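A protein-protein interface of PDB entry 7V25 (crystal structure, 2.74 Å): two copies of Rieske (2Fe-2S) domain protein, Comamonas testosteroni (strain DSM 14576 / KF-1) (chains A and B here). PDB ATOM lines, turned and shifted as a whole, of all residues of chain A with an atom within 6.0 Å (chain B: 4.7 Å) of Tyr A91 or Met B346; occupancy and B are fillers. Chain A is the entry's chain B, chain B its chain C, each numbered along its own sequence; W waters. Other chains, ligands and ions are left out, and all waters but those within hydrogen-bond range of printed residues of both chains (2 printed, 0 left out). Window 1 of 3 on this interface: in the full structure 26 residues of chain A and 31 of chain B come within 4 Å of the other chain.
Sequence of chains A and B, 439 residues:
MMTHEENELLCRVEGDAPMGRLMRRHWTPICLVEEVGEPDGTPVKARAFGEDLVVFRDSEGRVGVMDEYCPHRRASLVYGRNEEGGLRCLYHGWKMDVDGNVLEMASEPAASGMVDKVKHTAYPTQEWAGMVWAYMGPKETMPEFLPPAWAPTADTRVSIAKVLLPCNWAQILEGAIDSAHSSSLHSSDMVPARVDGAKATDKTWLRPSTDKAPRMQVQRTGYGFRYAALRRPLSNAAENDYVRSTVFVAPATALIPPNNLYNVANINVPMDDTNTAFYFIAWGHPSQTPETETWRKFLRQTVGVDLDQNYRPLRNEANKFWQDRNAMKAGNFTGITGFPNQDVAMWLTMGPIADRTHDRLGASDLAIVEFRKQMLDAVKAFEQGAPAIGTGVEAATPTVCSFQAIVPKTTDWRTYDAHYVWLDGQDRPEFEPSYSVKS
Of the printed residues of chain B, Arg A73 touches Asp B178 and Met B350.
Of the printed residues of chain B, Leu A90 touches Ser B184 and Leu B185.
Of the printed residues of chain B, Tyr A91 touches Gly B175 (3.7 Å), His B181 (3.6 Å), Ser B184 (3.5 Å), Leu B185 (3.7 Å), Met B346 (3.7 Å), Trp B347 (3.1 Å) and Met B350 (3.1 Å).
Of the printed residues of chain B, Gly A93 touches Ser B184 (3.2 Å).
Met B346 touches two residues of chain A.
The nearest residue of chain A that does not touch Met B346 is Leu A90 (4.2 Å).
Among the printed residues, pairs that only touch across the chains: Arg A73 with Met B350, Ala A75 with Met B346, Ala A75 with Thr B349, Tyr A79 with Thr B349, Leu A90 with Ser B184, Tyr A91 with Gly B175, Tyr A91 with His B181, Tyr A91 with Ser B184, Tyr A91 with Leu B185, Tyr A91 with Met B346, Tyr A91 with Met B350, His A92 with His B181 and His A92 with Ser B184.
Water W1 lies within hydrogen-bond range of OH of Tyr A91 (3.1 Å), NH2 of Arg A73 (3.2 Å) and SD of Met B350 (3.7 Å).
Water W2 bridges O of Met B350 (3.3 Å) and O of Arg A74 (3.5 Å).
A ring nitrogen (ND1) of His B181 lies close to the backbone carbonyl oxygen (O) of Gly B175 (3.5 Å).
NH2 of Arg A73 is in hydrogen-bond range of OH of Tyr A91, 3.4 Å away.
O of Ala B345 lies within hydrogen-bond range of OG1 of Thr B349, 2.9 Å away.
NH1 of Arg A73 lies within hydrogen-bond range of NE2 of His A92 (3.1 Å).
O of Met B346 lies within hydrogen-bond range of OG1 of Thr B349.
The backbone carbonyl oxygen (O) of Asp B178 is in hydrogen-bond range of a ring nitrogen (ND1) of His B181.
No position is printed for both chains.
Of the 19 pairs that touch across the chains among the printed residues, none has its exchanged pair printed and touching as well.
A ring nitrogen (NE2) of His A92 lies within hydrogen-bond range of the side-chain carboxylate (OD2) of Asp B178 (2.7 Å).
O of Leu A90 lies close to N of Leu B185, at 3.2 Å.
The side-chain hydroxyl (OG1) of Thr B349 is in hydrogen-bond range of the backbone NH (N) of Ser A76 (3.1 Å).
The indole nitrogen of Trp B347 lies within hydrogen-bond range of the side-chain hydroxyl of Tyr A91.
The side-chain hydroxyl of Ser B184 is in hydrogen-bond range of the backbone NH of Gly A93.
The guanidinium group (NH1) of Arg A73 is in salt-bridge range of the side-chain carboxylate (OD2) of Asp B178, 3.1 Å away.
Of the 14 printed residues of chain B, 9 touch a printed residue of chain A.
Hydrophobic or aromatic side chains of chain A that line the printed part of chain B: Ala A75, Tyr A79, Leu A90, Tyr A91 and His A92.
Among the printed residues, Asp or Glu carboxylates within 4 Å of a Lys or Arg side-chain nitrogen of the other chain: Arg A73 with Asp B178.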
ATOM      1  N   HIS A  72      20.477 -20.794  25.044  1.00  0.00           N
ATOM      2  CA  HIS A  72      19.630 -20.857  26.218  1.00  0.00           C
ATOM      3  C   HIS A  72      18.418 -21.753  25.957  1.00  0.00           C
ATOM      4  O   HIS A  72      18.432 -22.936  26.332  1.00  0.00           O
ATOM      5  CB  HIS A  72      19.289 -19.453  26.719  1.00  0.00           C
ATOM      6  CG  HIS A  72      18.501 -19.484  27.983  1.00  0.00           C
ATOM      7  ND1 HIS A  72      17.537 -18.531  28.289  1.00  0.00           N
ATOM      8  CD2 HIS A  72      18.496 -20.369  29.004  1.00  0.00           C
ATOM      9  CE1 HIS A  72      16.993 -18.811  29.453  1.00  0.00           C
ATOM     10  NE2 HIS A  72      17.567 -19.933  29.906  1.00  0.00           N
ATOM     11  N   ARG A  73      17.376 -21.187  25.320  1.00  0.00           N
ATOM     12  CA  ARG A  73      16.099 -21.885  25.225  1.00  0.00           C
ATOM     13  C   ARG A  73      15.651 -22.076  23.772  1.00  0.00           C
ATOM     14  O   ARG A  73      14.550 -22.566  23.523  1.00  0.00           O
ATOM     15  CB  ARG A  73      15.064 -21.282  26.187  1.00  0.00           C
ATOM     16  CG  ARG A  73      14.446 -22.327  27.107  1.00  0.00           C
ATOM     17  CD  ARG A  73      13.885 -21.891  28.442  1.00  0.00           C
ATOM     18  NE  ARG A  73      12.541 -21.345  28.300  1.00  0.00           N
ATOM     19  CZ  ARG A  73      12.118 -20.208  28.852  1.00  0.00           C
ATOM     20  NH1 ARG A  73      12.926 -19.496  29.621  1.00  0.00           N
ATOM     21  NH2 ARG A  73      10.879 -19.792  28.659  1.00  0.00           N
ATOM     22  N   ARG A  74      16.529 -21.699  22.828  1.00  0.00           N
ATOM     23  CA  ARG A  74      16.497 -22.083  21.417  1.00  0.00           C
ATOM     24  C   ARG A  74      15.736 -21.076  20.547  1.00  0.00           C
ATOM     25  O   ARG A  74      15.533 -21.328  19.368  1.00  0.00           O
ATOM     26  CB  ARG A  74      16.069 -23.541  21.186  1.00  0.00           C
ATOM     27  CG  ARG A  74      16.891 -24.611  21.898  1.00  0.00           C
ATOM     28  CD  ARG A  74      18.324 -24.827  21.433  1.00  0.00           C
ATOM     29  NE  ARG A  74      18.433 -25.280  20.047  1.00  0.00           N
ATOM     30  CZ  ARG A  74      19.517 -25.154  19.275  1.00  0.00           C
ATOM     31  NH1 ARG A  74      20.620 -24.595  19.751  1.00  0.00           N
ATOM     32  NH2 ARG A  74      19.491 -25.584  18.023  1.00  0.00           N
ATOM     33  N   ALA A  75      15.366 -19.911  21.093  1.00  0.00           N
ATOM     34  CA  ALA A  75      14.767 -18.833  20.311  1.00  0.00           C
ATOM     35  C   ALA A  75      15.711 -18.381  19.189  1.00  0.00           C
ATOM     36  O   ALA A  75      16.913 -18.656  19.224  1.00  0.00           O
ATOM     37  CB  ALA A  75      14.434 -17.693  21.234  1.00  0.00           C
ATOM     38  N   SER A  76      15.169 -17.665  18.192  1.00  0.00           N
ATOM     39  CA  SER A  76      15.947 -17.310  17.011  1.00  0.00           C
ATOM     40  C   SER A  76      16.794 -16.065  17.240  1.00  0.00           C
ATOM     41  O   SER A  76      16.269 -14.972  17.438  1.00  0.00           O
ATOM     42  CB  SER A  76      15.095 -17.134  15.786  1.00  0.00           C
ATOM     43  OG  SER A  76      15.919 -16.723  14.713  1.00  0.00           O
ATOM     44  N   TYR A  79      16.548 -12.450  15.548  1.00  0.00           N
ATOM     45  CA  TYR A  79      15.715 -11.384  16.070  1.00  0.00           C
ATOM     46  C   TYR A  79      16.514 -10.469  17.004  1.00  0.00           C
ATOM     47  O   TYR A  79      15.993  -9.454  17.467  1.00  0.00           O
ATOM     48  CB  TYR A  79      14.440 -11.980  16.673  1.00  0.00           C
ATOM     49  CG  TYR A  79      13.509 -12.538  15.627  1.00  0.00           C
ATOM     50  CD1 TYR A  79      12.505 -11.758  15.070  1.00  0.00           C
ATOM     51  CD2 TYR A  79      13.665 -13.830  15.146  1.00  0.00           C
ATOM     52  CE1 TYR A  79      11.666 -12.252  14.084  1.00  0.00           C
ATOM     53  CE2 TYR A  79      12.828 -14.345  14.173  1.00  0.00           C
ATOM     54  CZ  TYR A  79      11.829 -13.550  13.635  1.00  0.00           C
ATOM     55  OH  TYR A  79      10.999 -14.046  12.664  1.00  0.00           O
ATOM     56  N   CYS A  89      20.379 -12.148  22.418  1.00  0.00           N
ATOM     57  CA  CYS A  89      19.048 -12.711  22.256  1.00  0.00           C
ATOM     58  C   CYS A  89      18.032 -11.728  22.853  1.00  0.00           C
ATOM     59  O   CYS A  89      18.376 -10.998  23.775  1.00  0.00           O
ATOM     60  CB  CYS A  89      19.014 -14.059  22.967  1.00  0.00           C
ATOM     61  SG  CYS A  89      17.569 -15.069  22.552  1.00  0.00           S
ATOM     62  N   LEU A  90      16.790 -11.684  22.340  1.00  0.00           N
ATOM     63  CA  LEU A  90      15.803 -10.760  22.885  1.00  0.00           C
ATOM     64  C   LEU A  90      15.200 -11.311  24.178  1.00  0.00           C
ATOM     65  O   LEU A  90      14.696 -10.549  25.003  1.00  0.00           O
ATOM     66  CB  LEU A  90      14.680 -10.484  21.873  1.00  0.00           C
ATOM     67  CG  LEU A  90      15.032  -9.767  20.563  1.00  0.00           C
ATOM     68  CD1 LEU A  90      13.764  -9.366  19.837  1.00  0.00           C
ATOM     69  CD2 LEU A  90      15.890  -8.527  20.768  1.00  0.00           C
ATOM     70  N   TYR A  91      15.209 -12.638  24.337  1.00  0.00           N
ATOM     71  CA  TYR A  91      14.340 -13.313  25.297  1.00  0.00           C
ATOM     72  C   TYR A  91      14.802 -13.080  26.735  1.00  0.00           C
ATOM     73  O   TYR A  91      13.990 -12.655  27.555  1.00  0.00           O
ATOM     74  CB  TYR A  91      14.282 -14.822  25.036  1.00  0.00           C
ATOM     75  CG  TYR A  91      13.009 -15.512  25.456  1.00  0.00           C
ATOM     76  CD1 TYR A  91      12.025 -14.850  26.174  1.00  0.00           C
ATOM     77  CD2 TYR A  91      12.790 -16.846  25.150  1.00  0.00           C
ATOM     78  CE1 TYR A  91      10.866 -15.501  26.579  1.00  0.00           C
ATOM     79  CE2 TYR A  91      11.630 -17.505  25.539  1.00  0.00           C
ATOM     80  CZ  TYR A  91      10.664 -16.834  26.265  1.00  0.00           C
ATOM     81  OH  TYR A  91       9.520 -17.476  26.656  1.00  0.00           O
ATOM     82  N   HIS A  92      16.080 -13.413  27.016  1.00  0.00           N
ATOM     83  CA  HIS A  92      16.706 -13.276  28.322  1.00  0.00           C
ATOM     84  C   HIS A  92      18.070 -12.602  28.192  1.00  0.00           C
ATOM     85  O   HIS A  92      18.831 -12.533  29.157  1.00  0.00           O
ATOM     86  CB  HIS A  92      16.858 -14.638  29.023  1.00  0.00           C
ATOM     87  CG  HIS A  92      15.638 -15.491  28.982  1.00  0.00           C
ATOM     88  ND1 HIS A  92      15.380 -16.362  27.937  1.00  0.00           N
ATOM     89  CD2 HIS A  92      14.594 -15.603  29.834  1.00  0.00           C
ATOM     90  CE1 HIS A  92      14.237 -16.982  28.154  1.00  0.00           C
ATOM     91  NE2 HIS A  92      13.735 -16.528  29.305  1.00  0.00           N
ATOM     92  N   GLY A  93      18.404 -12.145  26.987  1.00  0.00           N
ATOM     93  CA  GLY A  93      19.540 -11.254  26.825  1.00  0.00           C
ATOM     94  C   GLY A  93      20.917 -11.919  26.916  1.00  0.00           C
ATOM     95  O   GLY A  93      21.909 -11.210  27.097  1.00  0.00           O
ATOM     96  N   GLY B 175       6.553 -19.516  29.181  1.00  0.00           N
ATOM     97  CA  GLY B 175       6.714 -18.085  28.965  1.00  0.00           C
ATOM     98  C   GLY B 175       5.952 -17.235  29.980  1.00  0.00           C
ATOM     99  O   GLY B 175       6.380 -16.124  30.285  1.00  0.00           O
ATOM    100  N   ASP B 178       7.931 -17.033  33.687  1.00  0.00           N
ATOM    101  CA  ASP B 178       9.371 -16.890  33.599  1.00  0.00           C
ATOM    102  C   ASP B 178       9.761 -15.443  33.846  1.00  0.00           C
ATOM    103  O   ASP B 178       9.862 -14.672  32.911  1.00  0.00           O
ATOM    104  CB  ASP B 178       9.864 -17.464  32.266  1.00  0.00           C
ATOM    105  CG  ASP B 178      11.274 -17.051  31.882  1.00  0.00           C
ATOM    106  OD1 ASP B 178      12.130 -16.856  32.788  1.00  0.00           O
ATOM    107  OD2 ASP B 178      11.496 -16.920  30.682  1.00  0.00           O
ATOM    108  N   HIS B 181      12.325 -12.799  32.014  1.00  0.00           N
ATOM    109  CA  HIS B 181      12.139 -12.446  30.618  1.00  0.00           C
ATOM    110  C   HIS B 181      11.621 -11.022  30.504  1.00  0.00           C
ATOM    111  O   HIS B 181      11.877 -10.366  29.492  1.00  0.00           O
ATOM    112  CB  HIS B 181      11.326 -13.502  29.845  1.00  0.00           C
ATOM    113  CG  HIS B 181       9.859 -13.250  29.677  1.00  0.00           C
ATOM    114  ND1 HIS B 181       8.918 -13.737  30.556  1.00  0.00           N
ATOM    115  CD2 HIS B 181       9.158 -12.650  28.688  1.00  0.00           C
ATOM    116  CE1 HIS B 181       7.708 -13.430  30.141  1.00  0.00           C
ATOM    117  NE2 HIS B 181       7.826 -12.765  28.993  1.00  0.00           N
ATOM    118  N   SER B 184      14.304  -8.421  30.058  1.00  0.00           N
ATOM    119  CA  SER B 184      14.956  -8.451  28.760  1.00  0.00           C
ATOM    120  C   SER B 184      13.938  -8.118  27.666  1.00  0.00           C
ATOM    121  O   SER B 184      13.877  -6.985  27.186  1.00  0.00           O
ATOM    122  CB  SER B 184      15.663  -9.760  28.537  1.00  0.00           C
ATOM    123  OG  SER B 184      16.971  -9.525  28.034  1.00  0.00           O
ATOM    124  N   LEU B 185      13.094  -9.090  27.316  1.00  0.00           N
ATOM    125  CA  LEU B 185      12.238  -8.985  26.143  1.00  0.00           C
ATOM    126  C   LEU B 185      11.312  -7.769  26.256  1.00  0.00           C
ATOM    127  O   LEU B 185      11.194  -6.993  25.305  1.00  0.00           O
ATOM    128  CB  LEU B 185      11.466 -10.301  25.973  1.00  0.00           C
ATOM    129  CG  LEU B 185      10.677 -10.481  24.677  1.00  0.00           C
ATOM    130  CD1 LEU B 185      11.614 -10.821  23.527  1.00  0.00           C
ATOM    131  CD2 LEU B 185       9.636 -11.576  24.837  1.00  0.00           C
ATOM    132  N   GLN B 342       5.945  -9.779  21.248  1.00  0.00           N
ATOM    133  CA  GLN B 342       7.345 -10.059  21.503  1.00  0.00           C
ATOM    134  C   GLN B 342       7.494 -11.498  21.996  1.00  0.00           C
ATOM    135  O   GLN B 342       8.421 -12.205  21.601  1.00  0.00           O
ATOM    136  CB  GLN B 342       7.866  -9.108  22.579  1.00  0.00           C
ATOM    137  CG  GLN B 342       8.053  -7.668  22.116  1.00  0.00           C
ATOM    138  CD  GLN B 342       7.659  -6.655  23.169  1.00  0.00           C
ATOM    139  OE1 GLN B 342       7.465  -6.979  24.344  1.00  0.00           O
ATOM    140  NE2 GLN B 342       7.523  -5.409  22.746  1.00  0.00           N
ATOM    141  N   ASP B 343       6.592 -11.914  22.895  1.00  0.00           N
ATOM    142  CA  ASP B 343       6.555 -13.275  23.406  1.00  0.00           C
ATOM    143  C   ASP B 343       6.398 -14.239  22.224  1.00  0.00           C
ATOM    144  O   ASP B 343       7.216 -15.146  22.070  1.00  0.00           O
ATOM    145  CB  ASP B 343       5.510 -13.450  24.521  1.00  0.00           C
ATOM    146  CG  ASP B 343       5.918 -13.022  25.935  1.00  0.00           C
ATOM    147  OD1 ASP B 343       5.095 -12.336  26.605  1.00  0.00           O
ATOM    148  OD2 ASP B 343       7.021 -13.415  26.398  1.00  0.00           O
ATOM    149  N   VAL B 344       5.402 -13.996  21.350  1.00  0.00           N
ATOM    150  CA  VAL B 344       5.030 -14.923  20.283  1.00  0.00           C
ATOM    151  C   VAL B 344       6.240 -15.290  19.409  1.00  0.00           C
ATOM    152  O   VAL B 344       6.434 -16.465  19.080  1.00  0.00           O
ATOM    153  CB  VAL B 344       3.810 -14.432  19.473  1.00  0.00           C
ATOM    154  CG1 VAL B 344       3.651 -15.172  18.158  1.00  0.00           C
ATOM    155  CG2 VAL B 344       2.520 -14.553  20.258  1.00  0.00           C
ATOM    156  N   ALA B 345       7.061 -14.293  19.048  1.00  0.00           N
ATOM    157  CA  ALA B 345       8.195 -14.484  18.162  1.00  0.00           C
ATOM    158  C   ALA B 345       9.209 -15.421  18.804  1.00  0.00           C
ATOM    159  O   ALA B 345       9.817 -16.261  18.140  1.00  0.00           O
ATOM    160  CB  ALA B 345       8.830 -13.157  17.866  1.00  0.00           C
ATOM    161  N   MET B 346       9.415 -15.258  20.110  1.00  0.00           N
ATOM    162  CA  MET B 346      10.319 -16.162  20.799  1.00  0.00           C
ATOM    163  C   MET B 346       9.734 -17.566  20.741  1.00  0.00           C
ATOM    164  O   MET B 346      10.418 -18.495  20.330  1.00  0.00           O
ATOM    165  CB  MET B 346      10.574 -15.734  22.249  1.00  0.00           C
ATOM    166  CG  MET B 346      11.224 -14.358  22.378  1.00  0.00           C
ATOM    167  SD  MET B 346      12.801 -14.205  21.481  1.00  0.00           S
ATOM    168  CE  MET B 346      12.244 -13.677  19.860  1.00  0.00           C
ATOM    169  N   TRP B 347       8.459 -17.692  21.108  1.00  0.00           N
ATOM    170  CA  TRP B 347       7.844 -19.000  21.275  1.00  0.00           C
ATOM    171  C   TRP B 347       7.821 -19.763  19.952  1.00  0.00           C
ATOM    172  O   TRP B 347       8.119 -20.952  19.912  1.00  0.00           O
ATOM    173  CB  TRP B 347       6.420 -18.888  21.844  1.00  0.00           C
ATOM    174  CG  TRP B 347       6.293 -18.290  23.213  1.00  0.00           C
ATOM    175  CD1 TRP B 347       7.217 -18.292  24.217  1.00  0.00           C
ATOM    176  CD2 TRP B 347       5.133 -17.623  23.736  1.00  0.00           C
ATOM    177  NE1 TRP B 347       6.716 -17.664  25.320  1.00  0.00           N
ATOM    178  CE2 TRP B 347       5.433 -17.258  25.061  1.00  0.00           C
ATOM    179  CE3 TRP B 347       3.881 -17.288  23.210  1.00  0.00           C
ATOM    180  CZ2 TRP B 347       4.522 -16.567  25.863  1.00  0.00           C
ATOM    181  CZ3 TRP B 347       2.979 -16.622  24.008  1.00  0.00           C
ATOM    182  CH2 TRP B 347       3.292 -16.274  25.322  1.00  0.00           C
ATOM    183  N   LEU B 348       7.425 -19.074  18.883  1.00  0.00           N
ATOM    184  CA  LEU B 348       7.201 -19.734  17.616  1.00  0.00           C
ATOM    185  C   LEU B 348       8.525 -20.211  17.035  1.00  0.00           C
ATOM    186  O   LEU B 348       8.579 -21.292  16.456  1.00  0.00           O
ATOM    187  CB  LEU B 348       6.490 -18.771  16.662  1.00  0.00           C
ATOM    188  CG  LEU B 348       4.984 -18.615  16.870  1.00  0.00           C
ATOM    189  CD1 LEU B 348       4.288 -18.291  15.550  1.00  0.00           C
ATOM    190  CD2 LEU B 348       4.359 -19.852  17.522  1.00  0.00           C
ATOM    191  N   THR B 349       9.581 -19.415  17.197  1.00  0.00           N
ATOM    192  CA  THR B 349      10.842 -19.730  16.552  1.00  0.00           C
ATOM    193  C   THR B 349      11.558 -20.859  17.287  1.00  0.00           C
ATOM    194  O   THR B 349      12.492 -21.449  16.751  1.00  0.00           O
ATOM    195  CB  THR B 349      11.725 -18.487  16.408  1.00  0.00           C
ATOM    196  OG1 THR B 349      12.083 -18.024  17.711  1.00  0.00           O
ATOM    197  CG2 THR B 349      11.065 -17.400  15.589  1.00  0.00           C
ATOM    198  N   MET B 350      11.116 -21.148  18.515  1.00  0.00           N
ATOM    199  CA  MET B 350      11.546 -22.328  19.252  1.00  0.00           C
ATOM    200  C   MET B 350      11.183 -23.618  18.504  1.00  0.00           C
ATOM    201  O   MET B 350      11.734 -24.678  18.810  1.00  0.00           O
ATOM    202  CB  MET B 350      10.880 -22.368  20.628  1.00  0.00           C
ATOM    203  CG  MET B 350      11.750 -21.806  21.704  1.00  0.00           C
ATOM    204  SD  MET B 350      10.849 -21.466  23.246  1.00  0.00           S
ATOM    205  CE  MET B 350      11.776 -20.019  23.747  1.00  0.00           C
HETATM  206  O   HOH W   1       8.836 -20.431  26.226  1.00  0.00           O
HETATM  207  O   HOH W   2      14.728 -24.149  17.515  1.00  0.00           O
